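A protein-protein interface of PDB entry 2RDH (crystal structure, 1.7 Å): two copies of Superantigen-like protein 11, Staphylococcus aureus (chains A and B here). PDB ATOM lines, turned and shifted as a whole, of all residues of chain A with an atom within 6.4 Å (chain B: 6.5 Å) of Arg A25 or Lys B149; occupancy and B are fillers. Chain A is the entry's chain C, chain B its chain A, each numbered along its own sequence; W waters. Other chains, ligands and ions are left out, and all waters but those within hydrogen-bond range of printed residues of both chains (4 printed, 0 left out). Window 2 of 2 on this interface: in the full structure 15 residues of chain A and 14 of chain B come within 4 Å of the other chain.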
ATOM      1  N   ASP A  23     -19.635  15.057 -17.961  1.00  0.00           N
ATOM      2  CA  ASP A  23     -19.150  14.358 -16.799  1.00  0.00           C
ATOM      3  C   ASP A  23     -19.916  13.035 -16.754  1.00  0.00           C
ATOM      4  O   ASP A  23     -21.112  12.999 -16.417  1.00  0.00           O
ATOM      5  CB  ASP A  23     -19.366  15.279 -15.601  1.00  0.00           C
ATOM      6  CG  ASP A  23     -18.967  14.654 -14.281  1.00  0.00           C
ATOM      7  OD1 ASP A  23     -18.382  13.541 -14.270  1.00  0.00           O
ATOM      8  OD2 ASP A  23     -19.211  15.340 -13.259  1.00  0.00           O
ATOM      9  N   LEU A  24     -19.252  11.946 -17.182  1.00  0.00           N
ATOM     10  CA  LEU A  24     -19.902  10.619 -17.260  1.00  0.00           C
ATOM     11  C   LEU A  24     -19.520   9.799 -16.043  1.00  0.00           C
ATOM     12  O   LEU A  24     -18.319   9.696 -15.705  1.00  0.00           O
ATOM     13  CB  LEU A  24     -19.442   9.875 -18.528  1.00  0.00           C
ATOM     14  CG  LEU A  24     -19.519  10.616 -19.866  1.00  0.00           C
ATOM     15  CD1 LEU A  24     -19.075   9.695 -20.998  1.00  0.00           C
ATOM     16  CD2 LEU A  24     -20.934  11.145 -20.142  1.00  0.00           C
ATOM     17  N   ARG A  25     -20.539   9.242 -15.386  1.00  0.00           N
ATOM     18  CA  ARG A  25     -20.366   8.587 -14.091  1.00  0.00           C
ATOM     19  C   ARG A  25     -20.596   7.086 -14.125  1.00  0.00           C
ATOM     20  O   ARG A  25     -21.597   6.606 -14.685  1.00  0.00           O
ATOM     21  CB  ARG A  25     -21.305   9.185 -13.044  1.00  0.00           C
ATOM     22  CG  ARG A  25     -21.088  10.679 -12.717  1.00  0.00           C
ATOM     23  CD  ARG A  25     -19.619  10.993 -12.241  1.00  0.00           C
ATOM     24  NE  ARG A  25     -19.464  12.412 -11.850  1.00  0.00           N
ATOM     25  CZ  ARG A  25     -19.862  12.962 -10.701  1.00  0.00           C
ATOM     26  NH1 ARG A  25     -20.414  12.220  -9.734  1.00  0.00           N
ATOM     27  NH2 ARG A  25     -19.687  14.279 -10.507  1.00  0.00           N
ATOM     28  N   ASN A  26     -19.690   6.377 -13.454  1.00  0.00           N
ATOM     29  CA  ASN A  26     -19.829   4.945 -13.165  1.00  0.00           C
ATOM     30  C   ASN A  26     -20.037   4.070 -14.399  1.00  0.00           C
ATOM     31  O   ASN A  26     -21.079   3.407 -14.559  1.00  0.00           O
ATOM     32  CB  ASN A  26     -20.941   4.720 -12.140  1.00  0.00           C
ATOM     33  CG  ASN A  26     -20.942   3.307 -11.602  1.00  0.00           C
ATOM     34  OD1 ASN A  26     -19.906   2.686 -11.545  1.00  0.00           O
ATOM     35  ND2 ASN A  26     -22.105   2.790 -11.267  1.00  0.00           N
ATOM     36  N   LEU A  27     -19.053   4.066 -15.284  1.00  0.00           N
ATOM     37  CA  LEU A  27     -19.171   3.282 -16.511  1.00  0.00           C
ATOM     38  C   LEU A  27     -17.896   2.468 -16.817  1.00  0.00           C
ATOM     39  O   LEU A  27     -16.841   2.710 -16.209  1.00  0.00           O
ATOM     40  CB  LEU A  27     -19.586   4.204 -17.670  1.00  0.00           C
ATOM     41  CG  LEU A  27     -18.751   5.419 -18.082  1.00  0.00           C
ATOM     42  CD1 LEU A  27     -19.287   6.020 -19.366  1.00  0.00           C
ATOM     43  CD2 LEU A  27     -18.694   6.496 -17.015  1.00  0.00           C
ATOM     44  N   LEU A  65     -15.678   3.451 -13.646  1.00  0.00           N
ATOM     45  CA  LEU A  65     -14.879   4.644 -13.916  1.00  0.00           C
ATOM     46  C   LEU A  65     -15.786   5.849 -14.076  1.00  0.00           C
ATOM     47  O   LEU A  65     -16.945   5.700 -14.440  1.00  0.00           O
ATOM     48  CB  LEU A  65     -14.093   4.479 -15.215  1.00  0.00           C
ATOM     49  CG  LEU A  65     -13.003   3.396 -15.293  1.00  0.00           C
ATOM     50  CD1 LEU A  65     -12.419   3.323 -16.690  1.00  0.00           C
ATOM     51  CD2 LEU A  65     -11.906   3.646 -14.269  1.00  0.00           C
ATOM     52  N   ASP A  66     -15.270   7.024 -13.747  1.00  0.00           N
ATOM     53  CA  ASP A  66     -15.875   8.295 -14.216  1.00  0.00           C
ATOM     54  C   ASP A  66     -14.981   8.833 -15.309  1.00  0.00           C
ATOM     55  O   ASP A  66     -13.757   8.596 -15.300  1.00  0.00           O
ATOM     56  CB  ASP A  66     -15.959   9.329 -13.099  1.00  0.00           C
ATOM     57  CG  ASP A  66     -16.928   8.951 -11.975  1.00  0.00           C
ATOM     58  OD1 ASP A  66     -17.759   8.018 -12.121  1.00  0.00           O
ATOM     59  OD2 ASP A  66     -16.848   9.622 -10.917  1.00  0.00           O
ATOM     60  N   VAL A  67     -15.558   9.606 -16.226  1.00  0.00           N
ATOM     61  CA  VAL A  67     -14.739  10.260 -17.241  1.00  0.00           C
ATOM     62  C   VAL A  67     -15.248  11.665 -17.484  1.00  0.00           C
ATOM     63  O   VAL A  67     -16.447  11.887 -17.695  1.00  0.00           O
ATOM     64  CB  VAL A  67     -14.644   9.425 -18.558  1.00  0.00           C
ATOM     65  CG1 VAL A  67     -15.986   9.111 -19.118  1.00  0.00           C
ATOM     66  CG2 VAL A  67     -13.750  10.107 -19.632  1.00  0.00           C
ATOM     67  N   THR A  89     -14.600   5.831  -9.891  1.00  0.00           N
ATOM     68  CA  THR A  89     -15.864   6.432  -9.478  1.00  0.00           C
ATOM     69  C   THR A  89     -15.920   6.464  -7.945  1.00  0.00           C
ATOM     70  O   THR A  89     -15.145   5.749  -7.288  1.00  0.00           O
ATOM     71  CB  THR A  89     -17.058   5.658 -10.111  1.00  0.00           C
ATOM     72  OG1 THR A  89     -18.234   6.486 -10.166  1.00  0.00           O
ATOM     73  CG2 THR A  89     -17.334   4.345  -9.360  1.00  0.00           C
ATOM     74  N   ASN A  90     -16.804   7.281  -7.372  1.00  0.00           N
ATOM     75  CA  ASN A  90     -17.047   7.244  -5.917  1.00  0.00           C
ATOM     76  C   ASN A  90     -17.469   5.865  -5.410  1.00  0.00           C
ATOM     77  O   ASN A  90     -18.047   5.054  -6.141  1.00  0.00           O
ATOM     78  CB  ASN A  90     -18.089   8.284  -5.497  1.00  0.00           C
ATOM     79  CG  ASN A  90     -17.568   9.728  -5.610  1.00  0.00           C
ATOM     80  OD1 ASN A  90     -16.383   9.962  -5.875  1.00  0.00           O
ATOM     81  ND2 ASN A  90     -18.470  10.705  -5.413  1.00  0.00           N
ATOM     82  N   GLN A  93     -22.900   5.891  -5.461  1.00  0.00           N
ATOM     83  CA  GLN A  93     -23.360   6.916  -6.418  1.00  0.00           C
ATOM     84  C   GLN A  93     -24.215   7.996  -5.767  1.00  0.00           C
ATOM     85  O   GLN A  93     -24.742   8.873  -6.473  1.00  0.00           O
ATOM     86  CB  GLN A  93     -24.110   6.289  -7.605  1.00  0.00           C
ATOM     87  CG  GLN A  93     -23.260   5.412  -8.496  1.00  0.00           C
ATOM     88  CD  GLN A  93     -22.033   6.119  -9.022  1.00  0.00           C
ATOM     89  OE1 GLN A  93     -22.135   7.064  -9.821  1.00  0.00           O
ATOM     90  NE2 GLN A  93     -20.854   5.664  -8.582  1.00  0.00           N
ATOM     91  N   ILE A  95     -24.949  11.401  -3.765  1.00  0.00           N
ATOM     92  CA  ILE A  95     -24.284  12.703  -3.911  1.00  0.00           C
ATOM     93  C   ILE A  95     -23.883  13.206  -2.523  1.00  0.00           C
ATOM     94  O   ILE A  95     -24.729  13.277  -1.618  1.00  0.00           O
ATOM     95  CB  ILE A  95     -25.175  13.741  -4.600  1.00  0.00           C
ATOM     96  CG1 ILE A  95     -25.399  13.355  -6.066  1.00  0.00           C
ATOM     97  CG2 ILE A  95     -24.492  15.157  -4.534  1.00  0.00           C
ATOM     98  CD1 ILE A  95     -26.674  13.937  -6.659  1.00  0.00           C
ATOM     99  N   TYR A 124     -17.105  17.089  -5.228  1.00  0.00           N
ATOM    100  CA  TYR A 124     -18.040  15.970  -5.021  1.00  0.00           C
ATOM    101  C   TYR A 124     -17.445  14.617  -5.405  1.00  0.00           C
ATOM    102  O   TYR A 124     -18.132  13.593  -5.303  1.00  0.00           O
ATOM    103  CB  TYR A 124     -19.301  16.198  -5.850  1.00  0.00           C
ATOM    104  CG  TYR A 124     -19.978  17.524  -5.603  1.00  0.00           C
ATOM    105  CD1 TYR A 124     -19.833  18.584  -6.510  1.00  0.00           C
ATOM    106  CD2 TYR A 124     -20.792  17.704  -4.494  1.00  0.00           C
ATOM    107  CE1 TYR A 124     -20.484  19.803  -6.287  1.00  0.00           C
ATOM    108  CE2 TYR A 124     -21.441  18.915  -4.265  1.00  0.00           C
ATOM    109  CZ  TYR A 124     -21.275  19.955  -5.166  1.00  0.00           C
ATOM    110  OH  TYR A 124     -21.929  21.155  -4.949  1.00  0.00           O
ATOM    111  N   LYS A 125     -16.192  14.616  -5.870  1.00  0.00           N
ATOM    112  CA  LYS A 125     -15.503  13.385  -6.286  1.00  0.00           C
ATOM    113  C   LYS A 125     -14.320  13.048  -5.401  1.00  0.00           C
ATOM    114  O   LYS A 125     -13.497  13.904  -5.094  1.00  0.00           O
ATOM    115  CB  LYS A 125     -15.063  13.463  -7.768  1.00  0.00           C
ATOM    116  CG  LYS A 125     -16.190  13.088  -8.736  1.00  0.00           C
ATOM    117  CD  LYS A 125     -15.833  13.166 -10.200  1.00  0.00           C
ATOM    118  CE  LYS A 125     -14.625  12.355 -10.613  1.00  0.00           C
ATOM    119  NZ  LYS A 125     -14.581  10.942 -10.089  1.00  0.00           N
ATOM    120  N   GLU A 132     -10.540  18.011 -14.957  1.00  0.00           N
ATOM    121  CA  GLU A 132     -11.813  18.464 -14.447  1.00  0.00           C
ATOM    122  C   GLU A 132     -11.646  19.728 -13.621  1.00  0.00           C
ATOM    123  O   GLU A 132     -12.429  20.669 -13.781  1.00  0.00           O
ATOM    124  CB  GLU A 132     -12.478  17.387 -13.572  1.00  0.00           C
ATOM    125  CG  GLU A 132     -13.890  17.824 -13.135  1.00  0.00           C
ATOM    126  CD  GLU A 132     -14.752  16.759 -12.517  1.00  0.00           C
ATOM    127  OE1 GLU A 132     -14.490  15.540 -12.671  1.00  0.00           O
ATOM    128  OE2 GLU A 132     -15.749  17.179 -11.888  1.00  0.00           O
ATOM    129  N   ARG B   6     -31.553   3.056  -8.739  1.00  0.00           N
ATOM    130  CA  ARG B   6     -31.413   3.756 -10.054  1.00  0.00           C
ATOM    131  C   ARG B   6     -32.125   2.980 -11.135  1.00  0.00           C
ATOM    132  O   ARG B   6     -31.846   1.777 -11.347  1.00  0.00           O
ATOM    133  CB  ARG B   6     -29.950   3.914 -10.451  1.00  0.00           C
ATOM    134  CG  ARG B   6     -29.759   4.762 -11.705  1.00  0.00           C
ATOM    135  CD  ARG B   6     -28.276   5.025 -11.958  1.00  0.00           C
ATOM    136  NE  ARG B   6     -28.048   5.898 -13.107  1.00  0.00           N
ATOM    137  CZ  ARG B   6     -28.342   7.188 -13.136  1.00  0.00           C
ATOM    138  NH1 ARG B   6     -28.907   7.779 -12.081  1.00  0.00           N
ATOM    139  NH2 ARG B   6     -28.073   7.887 -14.235  1.00  0.00           N
ATOM    140  N   THR B  10     -33.937   6.144 -16.014  1.00  0.00           N
ATOM    141  CA  THR B  10     -33.148   7.348 -15.659  1.00  0.00           C
ATOM    142  C   THR B  10     -31.775   7.331 -16.335  1.00  0.00           C
ATOM    143  O   THR B  10     -31.358   8.312 -16.943  1.00  0.00           O
ATOM    144  CB  THR B  10     -33.043   7.493 -14.131  1.00  0.00           C
ATOM    145  OG1 THR B  10     -34.367   7.695 -13.630  1.00  0.00           O
ATOM    146  CG2 THR B  10     -32.136   8.685 -13.699  1.00  0.00           C
ATOM    147  N   GLN B  11     -31.091   6.193 -16.243  1.00  0.00           N
ATOM    148  CA  GLN B  11     -29.849   5.987 -16.967  1.00  0.00           C
ATOM    149  C   GLN B  11     -29.992   6.316 -18.455  1.00  0.00           C
ATOM    150  O   GLN B  11     -29.133   7.012 -19.014  1.00  0.00           O
ATOM    151  CB  GLN B  11     -29.334   4.567 -16.729  1.00  0.00           C
ATOM    152  CG  GLN B  11     -27.923   4.279 -17.284  1.00  0.00           C
ATOM    153  CD  GLN B  11     -26.843   5.289 -16.842  1.00  0.00           C
ATOM    154  OE1 GLN B  11     -26.789   5.724 -15.687  1.00  0.00           O
ATOM    155  NE2 GLN B  11     -25.960   5.648 -17.783  1.00  0.00           N
ATOM    156  N   SER B  14     -30.218  10.072 -19.000  1.00  0.00           N
ATOM    157  CA  SER B  14     -28.878  10.632 -18.797  1.00  0.00           C
ATOM    158  C   SER B  14     -28.041  10.470 -20.064  1.00  0.00           C
ATOM    159  O   SER B  14     -27.432  11.452 -20.586  1.00  0.00           O
ATOM    160  CB  SER B  14     -28.230   9.902 -17.628  1.00  0.00           C
ATOM    161  OG  SER B  14     -27.081  10.563 -17.199  1.00  0.00           O
ATOM    162  N   ASN B  18     -27.108  13.796 -22.053  1.00  0.00           N
ATOM    163  CA  ASN B  18     -25.728  14.245 -21.712  1.00  0.00           C
ATOM    164  C   ASN B  18     -24.729  13.952 -22.859  1.00  0.00           C
ATOM    165  O   ASN B  18     -23.795  13.144 -22.706  1.00  0.00           O
ATOM    166  CB  ASN B  18     -25.268  13.665 -20.355  1.00  0.00           C
ATOM    167  CG  ASN B  18     -24.053  14.443 -19.748  1.00  0.00           C
ATOM    168  OD1 ASN B  18     -23.763  15.584 -20.138  1.00  0.00           O
ATOM    169  ND2 ASN B  18     -23.384  13.832 -18.777  1.00  0.00           N
ATOM    170  N   ILE B 142     -28.347  19.008 -15.887  1.00  0.00           N
ATOM    171  CA  ILE B 142     -27.426  17.908 -15.707  1.00  0.00           C
ATOM    172  C   ILE B 142     -26.097  18.440 -15.158  1.00  0.00           C
ATOM    173  O   ILE B 142     -25.530  17.863 -14.239  1.00  0.00           O
ATOM    174  CB  ILE B 142     -27.254  17.177 -17.054  1.00  0.00           C
ATOM    175  CG1 ILE B 142     -28.509  16.337 -17.318  1.00  0.00           C
ATOM    176  CG2 ILE B 142     -25.961  16.298 -17.090  1.00  0.00           C
ATOM    177  CD1 ILE B 142     -28.516  15.766 -18.735  1.00  0.00           C
ATOM    178  N   ASP B 143     -25.652  19.544 -15.719  1.00  0.00           N
ATOM    179  CA  ASP B 143     -24.334  20.091 -15.340  1.00  0.00           C
ATOM    180  C   ASP B 143     -24.391  20.739 -13.965  1.00  0.00           C
ATOM    181  O   ASP B 143     -23.466  20.581 -13.164  1.00  0.00           O
ATOM    182  CB  ASP B 143     -23.899  21.144 -16.342  1.00  0.00           C
ATOM    183  CG  ASP B 143     -23.421  20.576 -17.645  1.00  0.00           C
ATOM    184  OD1 ASP B 143     -23.256  19.366 -17.759  1.00  0.00           O
ATOM    185  OD2 ASP B 143     -23.162  21.392 -18.575  1.00  0.00           O
ATOM    186  N   HIS B 145     -27.264  21.011 -11.658  1.00  0.00           N
ATOM    187  CA  HIS B 145     -28.330  20.680 -10.681  1.00  0.00           C
ATOM    188  C   HIS B 145     -28.582  19.190 -10.474  1.00  0.00           C
ATOM    189  O   HIS B 145     -29.670  18.756 -10.003  1.00  0.00           O
ATOM    190  CB  HIS B 145     -29.621  21.411 -11.039  1.00  0.00           C
ATOM    191  CG  HIS B 145     -29.507  22.900 -10.907  1.00  0.00           C
ATOM    192  ND1 HIS B 145     -29.497  23.531  -9.680  1.00  0.00           N
ATOM    193  CD2 HIS B 145     -29.407  23.885 -11.834  1.00  0.00           C
ATOM    194  CE1 HIS B 145     -29.388  24.838  -9.853  1.00  0.00           C
ATOM    195  NE2 HIS B 145     -29.318  25.082 -11.144  1.00  0.00           N
ATOM    196  N   ASP B 146     -27.551  18.419 -10.806  1.00  0.00           N
ATOM    197  CA  ASP B 146     -27.536  16.973 -10.585  1.00  0.00           C
ATOM    198  C   ASP B 146     -28.690  16.224 -11.252  1.00  0.00           C
ATOM    199  O   ASP B 146     -29.040  15.141 -10.812  1.00  0.00           O
ATOM    200  CB  ASP B 146     -27.492  16.628  -9.066  1.00  0.00           C
ATOM    201  CG  ASP B 146     -26.220  17.092  -8.396  1.00  0.00           C
ATOM    202  OD1 ASP B 146     -25.138  16.844  -8.948  1.00  0.00           O
ATOM    203  OD2 ASP B 146     -26.315  17.693  -7.303  1.00  0.00           O
ATOM    204  N   LEU B 147     -29.260  16.781 -12.312  1.00  0.00           N
ATOM    205  CA  LEU B 147     -30.338  16.080 -12.986  1.00  0.00           C
ATOM    206  C   LEU B 147     -29.886  14.688 -13.455  1.00  0.00           C
ATOM    207  O   LEU B 147     -28.794  14.520 -14.064  1.00  0.00           O
ATOM    208  CB  LEU B 147     -30.931  16.918 -14.144  1.00  0.00           C
ATOM    209  CG  LEU B 147     -32.111  16.259 -14.871  1.00  0.00           C
ATOM    210  CD1 LEU B 147     -33.346  16.302 -14.012  1.00  0.00           C
ATOM    211  CD2 LEU B 147     -32.375  17.054 -16.178  1.00  0.00           C
ATOM    212  N   TYR B 148     -30.718  13.691 -13.166  1.00  0.00           N
ATOM    213  CA  TYR B 148     -30.489  12.286 -13.571  1.00  0.00           C
ATOM    214  C   TYR B 148     -29.395  11.558 -12.772  1.00  0.00           C
ATOM    215  O   TYR B 148     -29.100  10.390 -13.047  1.00  0.00           O
ATOM    216  CB  TYR B 148     -30.367  12.123 -15.124  1.00  0.00           C
ATOM    217  CG  TYR B 148     -31.556  12.689 -15.894  1.00  0.00           C
ATOM    218  CD1 TYR B 148     -31.361  13.394 -17.094  1.00  0.00           C
ATOM    219  CD2 TYR B 148     -32.887  12.488 -15.446  1.00  0.00           C
ATOM    220  CE1 TYR B 148     -32.417  13.933 -17.797  1.00  0.00           C
ATOM    221  CE2 TYR B 148     -33.980  13.031 -16.151  1.00  0.00           C
ATOM    222  CZ  TYR B 148     -33.723  13.766 -17.333  1.00  0.00           C
ATOM    223  OH  TYR B 148     -34.758  14.316 -18.053  1.00  0.00           O
ATOM    224  N   LYS B 149     -28.877  12.217 -11.726  1.00  0.00           N
ATOM    225  CA  LYS B 149     -28.077  11.523 -10.704  1.00  0.00           C
ATOM    226  C   LYS B 149     -28.990  10.818  -9.705  1.00  0.00           C
ATOM    227  O   LYS B 149     -28.566   9.899  -8.963  1.00  0.00           O
ATOM    228  CB  LYS B 149     -27.131  12.480  -9.978  1.00  0.00           C
ATOM    229  CG  LYS B 149     -25.881  12.828 -10.838  1.00  0.00           C
ATOM    230  CD  LYS B 149     -24.876  13.633 -10.016  1.00  0.00           C
ATOM    231  CE  LYS B 149     -23.656  14.115 -10.809  1.00  0.00           C
ATOM    232  NZ  LYS B 149     -23.874  15.495 -11.350  1.00  0.00           N
ATOM    233  N   THR B 150     -30.246  11.241  -9.702  1.00  0.00           N
ATOM    234  CA  THR B 150     -31.289  10.619  -8.860  1.00  0.00           C
ATOM    235  C   THR B 150     -32.522  10.468  -9.759  1.00  0.00           C
ATOM    236  O   THR B 150     -32.570  11.043 -10.840  1.00  0.00           O
ATOM    237  CB  THR B 150     -31.652  11.513  -7.659  1.00  0.00           C
ATOM    238  OG1 THR B 150     -32.085  12.788  -8.145  1.00  0.00           O
ATOM    239  CG2 THR B 150     -30.446  11.713  -6.700  1.00  0.00           C
ATOM    240  N   GLU B 151     -33.516   9.699  -9.321  1.00  0.00           N
ATOM    241  CA  GLU B 151     -34.760   9.536 -10.092  1.00  0.00           C
ATOM    242  C   GLU B 151     -35.496  10.880 -10.213  1.00  0.00           C
ATOM    243  O   GLU B 151     -35.686  11.554  -9.191  1.00  0.00           O
ATOM    244  CB  GLU B 151     -35.665   8.523  -9.379  1.00  0.00           C
ATOM    245  CG  GLU B 151     -35.055   7.130  -9.247  1.00  0.00           C
ATOM    246  CD  GLU B 151     -34.644   6.592 -10.610  1.00  0.00           C
ATOM    247  OE1 GLU B 151     -35.532   6.436 -11.466  1.00  0.00           O
ATOM    248  OE2 GLU B 151     -33.433   6.371 -10.845  1.00  0.00           O
HETATM  249  O   HOH W   1     -27.340   9.784  -6.485  1.00  0.00           O
HETATM  250  O   HOH W   2     -23.172   7.359 -16.766  1.00  0.00           O
HETATM  251  O   HOH W   3     -22.066  16.599 -17.674  1.00  0.00           O
HETATM  252  O   HOH W   4     -21.500  16.402 -12.729  1.00  0.00           O
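Arg A25 touches just one residue of chain B: Lys B149 (3.9 Å). Lys B149 touches just these residues of chain A: Arg A25 (3.9 Å) and Ile A95 (3.7 Å). Of the printed residues of chain A, Asp B146 touches Ile A95. Printed residues of chain B within 4 Å of Ile A95: Asp B146 (3.6 Å) and Lys B149 (3.7 Å). Of the printed residues of chain B, Asp A23 touches Asn B18. Printed residues of chain A within 4 Å of Asn B18: Asp A23 (3.4 Å) and Leu A24 (3.9 Å). The nearest residue of chain B that does not touch Arg A25 is Gln B11 (5.4 Å). The nearest printed residue of chain B that does not touch Ile A95 is Thr B150 (4.4 Å).
Water W4 lies within hydrogen-bond range of the side-chain carboxylate (OD2) of Asp A23 (2.6 Å) and the side-chain amino group (NZ) of Lys B149 (2.9 Å). Water W2 lies within hydrogen-bond range of the backbone carbonyl oxygen (O) of Arg A25 and the side-chain amide nitrogen (NE2) of Gln B11. Water W1 lies within hydrogen-bond range of the backbone carbonyl oxygen of Gln A93 (2.8 Å) and the backbone carbonyl oxygen of Lys B149 (2.8 Å). Water W3 lies within hydrogen-bond range of N of Asp A23, OD1 of Asp B143 and OD1 of Asn B18.
No position is printed for both chains. Of the 5 pairs that touch across the chains among the printed residues, none has its exchanged pair printed and touching as well.
The side-chain amide nitrogen of Asn B18 is in hydrogen-bond range of the backbone carbonyl oxygen of Asp A23, 3.4 Å away.
Of the 14 printed residues of chain B, 3 touch a printed residue of chain A. Hydrophobic or aromatic side chains of chain A that line the printed part of chain B: Leu A24 and Ile A95. Among the printed residues, 5 pairs touch across the chains.
Leu A24 touches Asn B18. NH1 of Arg A25 touches CE of Lys B149, 3.9 Å away. Ile A95 touches Asp B146 (CD1 to CG, 3.6 Å). Lys B149 touches Ile A95.
The side-chain carboxylate (OD1) of Asp B146 lies within salt-bridge range of the side-chain amino group (NZ) of Lys B149 (3.0 Å). The side-chain carboxylate (OD1) of Asp A23 lies within salt-bridge range of the guanidinium group (NE) of Arg A25 (2.9 Å). The backbone carbonyl oxygen (O) of Leu A24 lies within hydrogen-bond range of the backbone NH (N) of Val A67, 2.8 Å away. The guanidinium group of Arg A25 is in salt-bridge range of the side-chain carboxylate of Asp A66 (3.9 Å).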
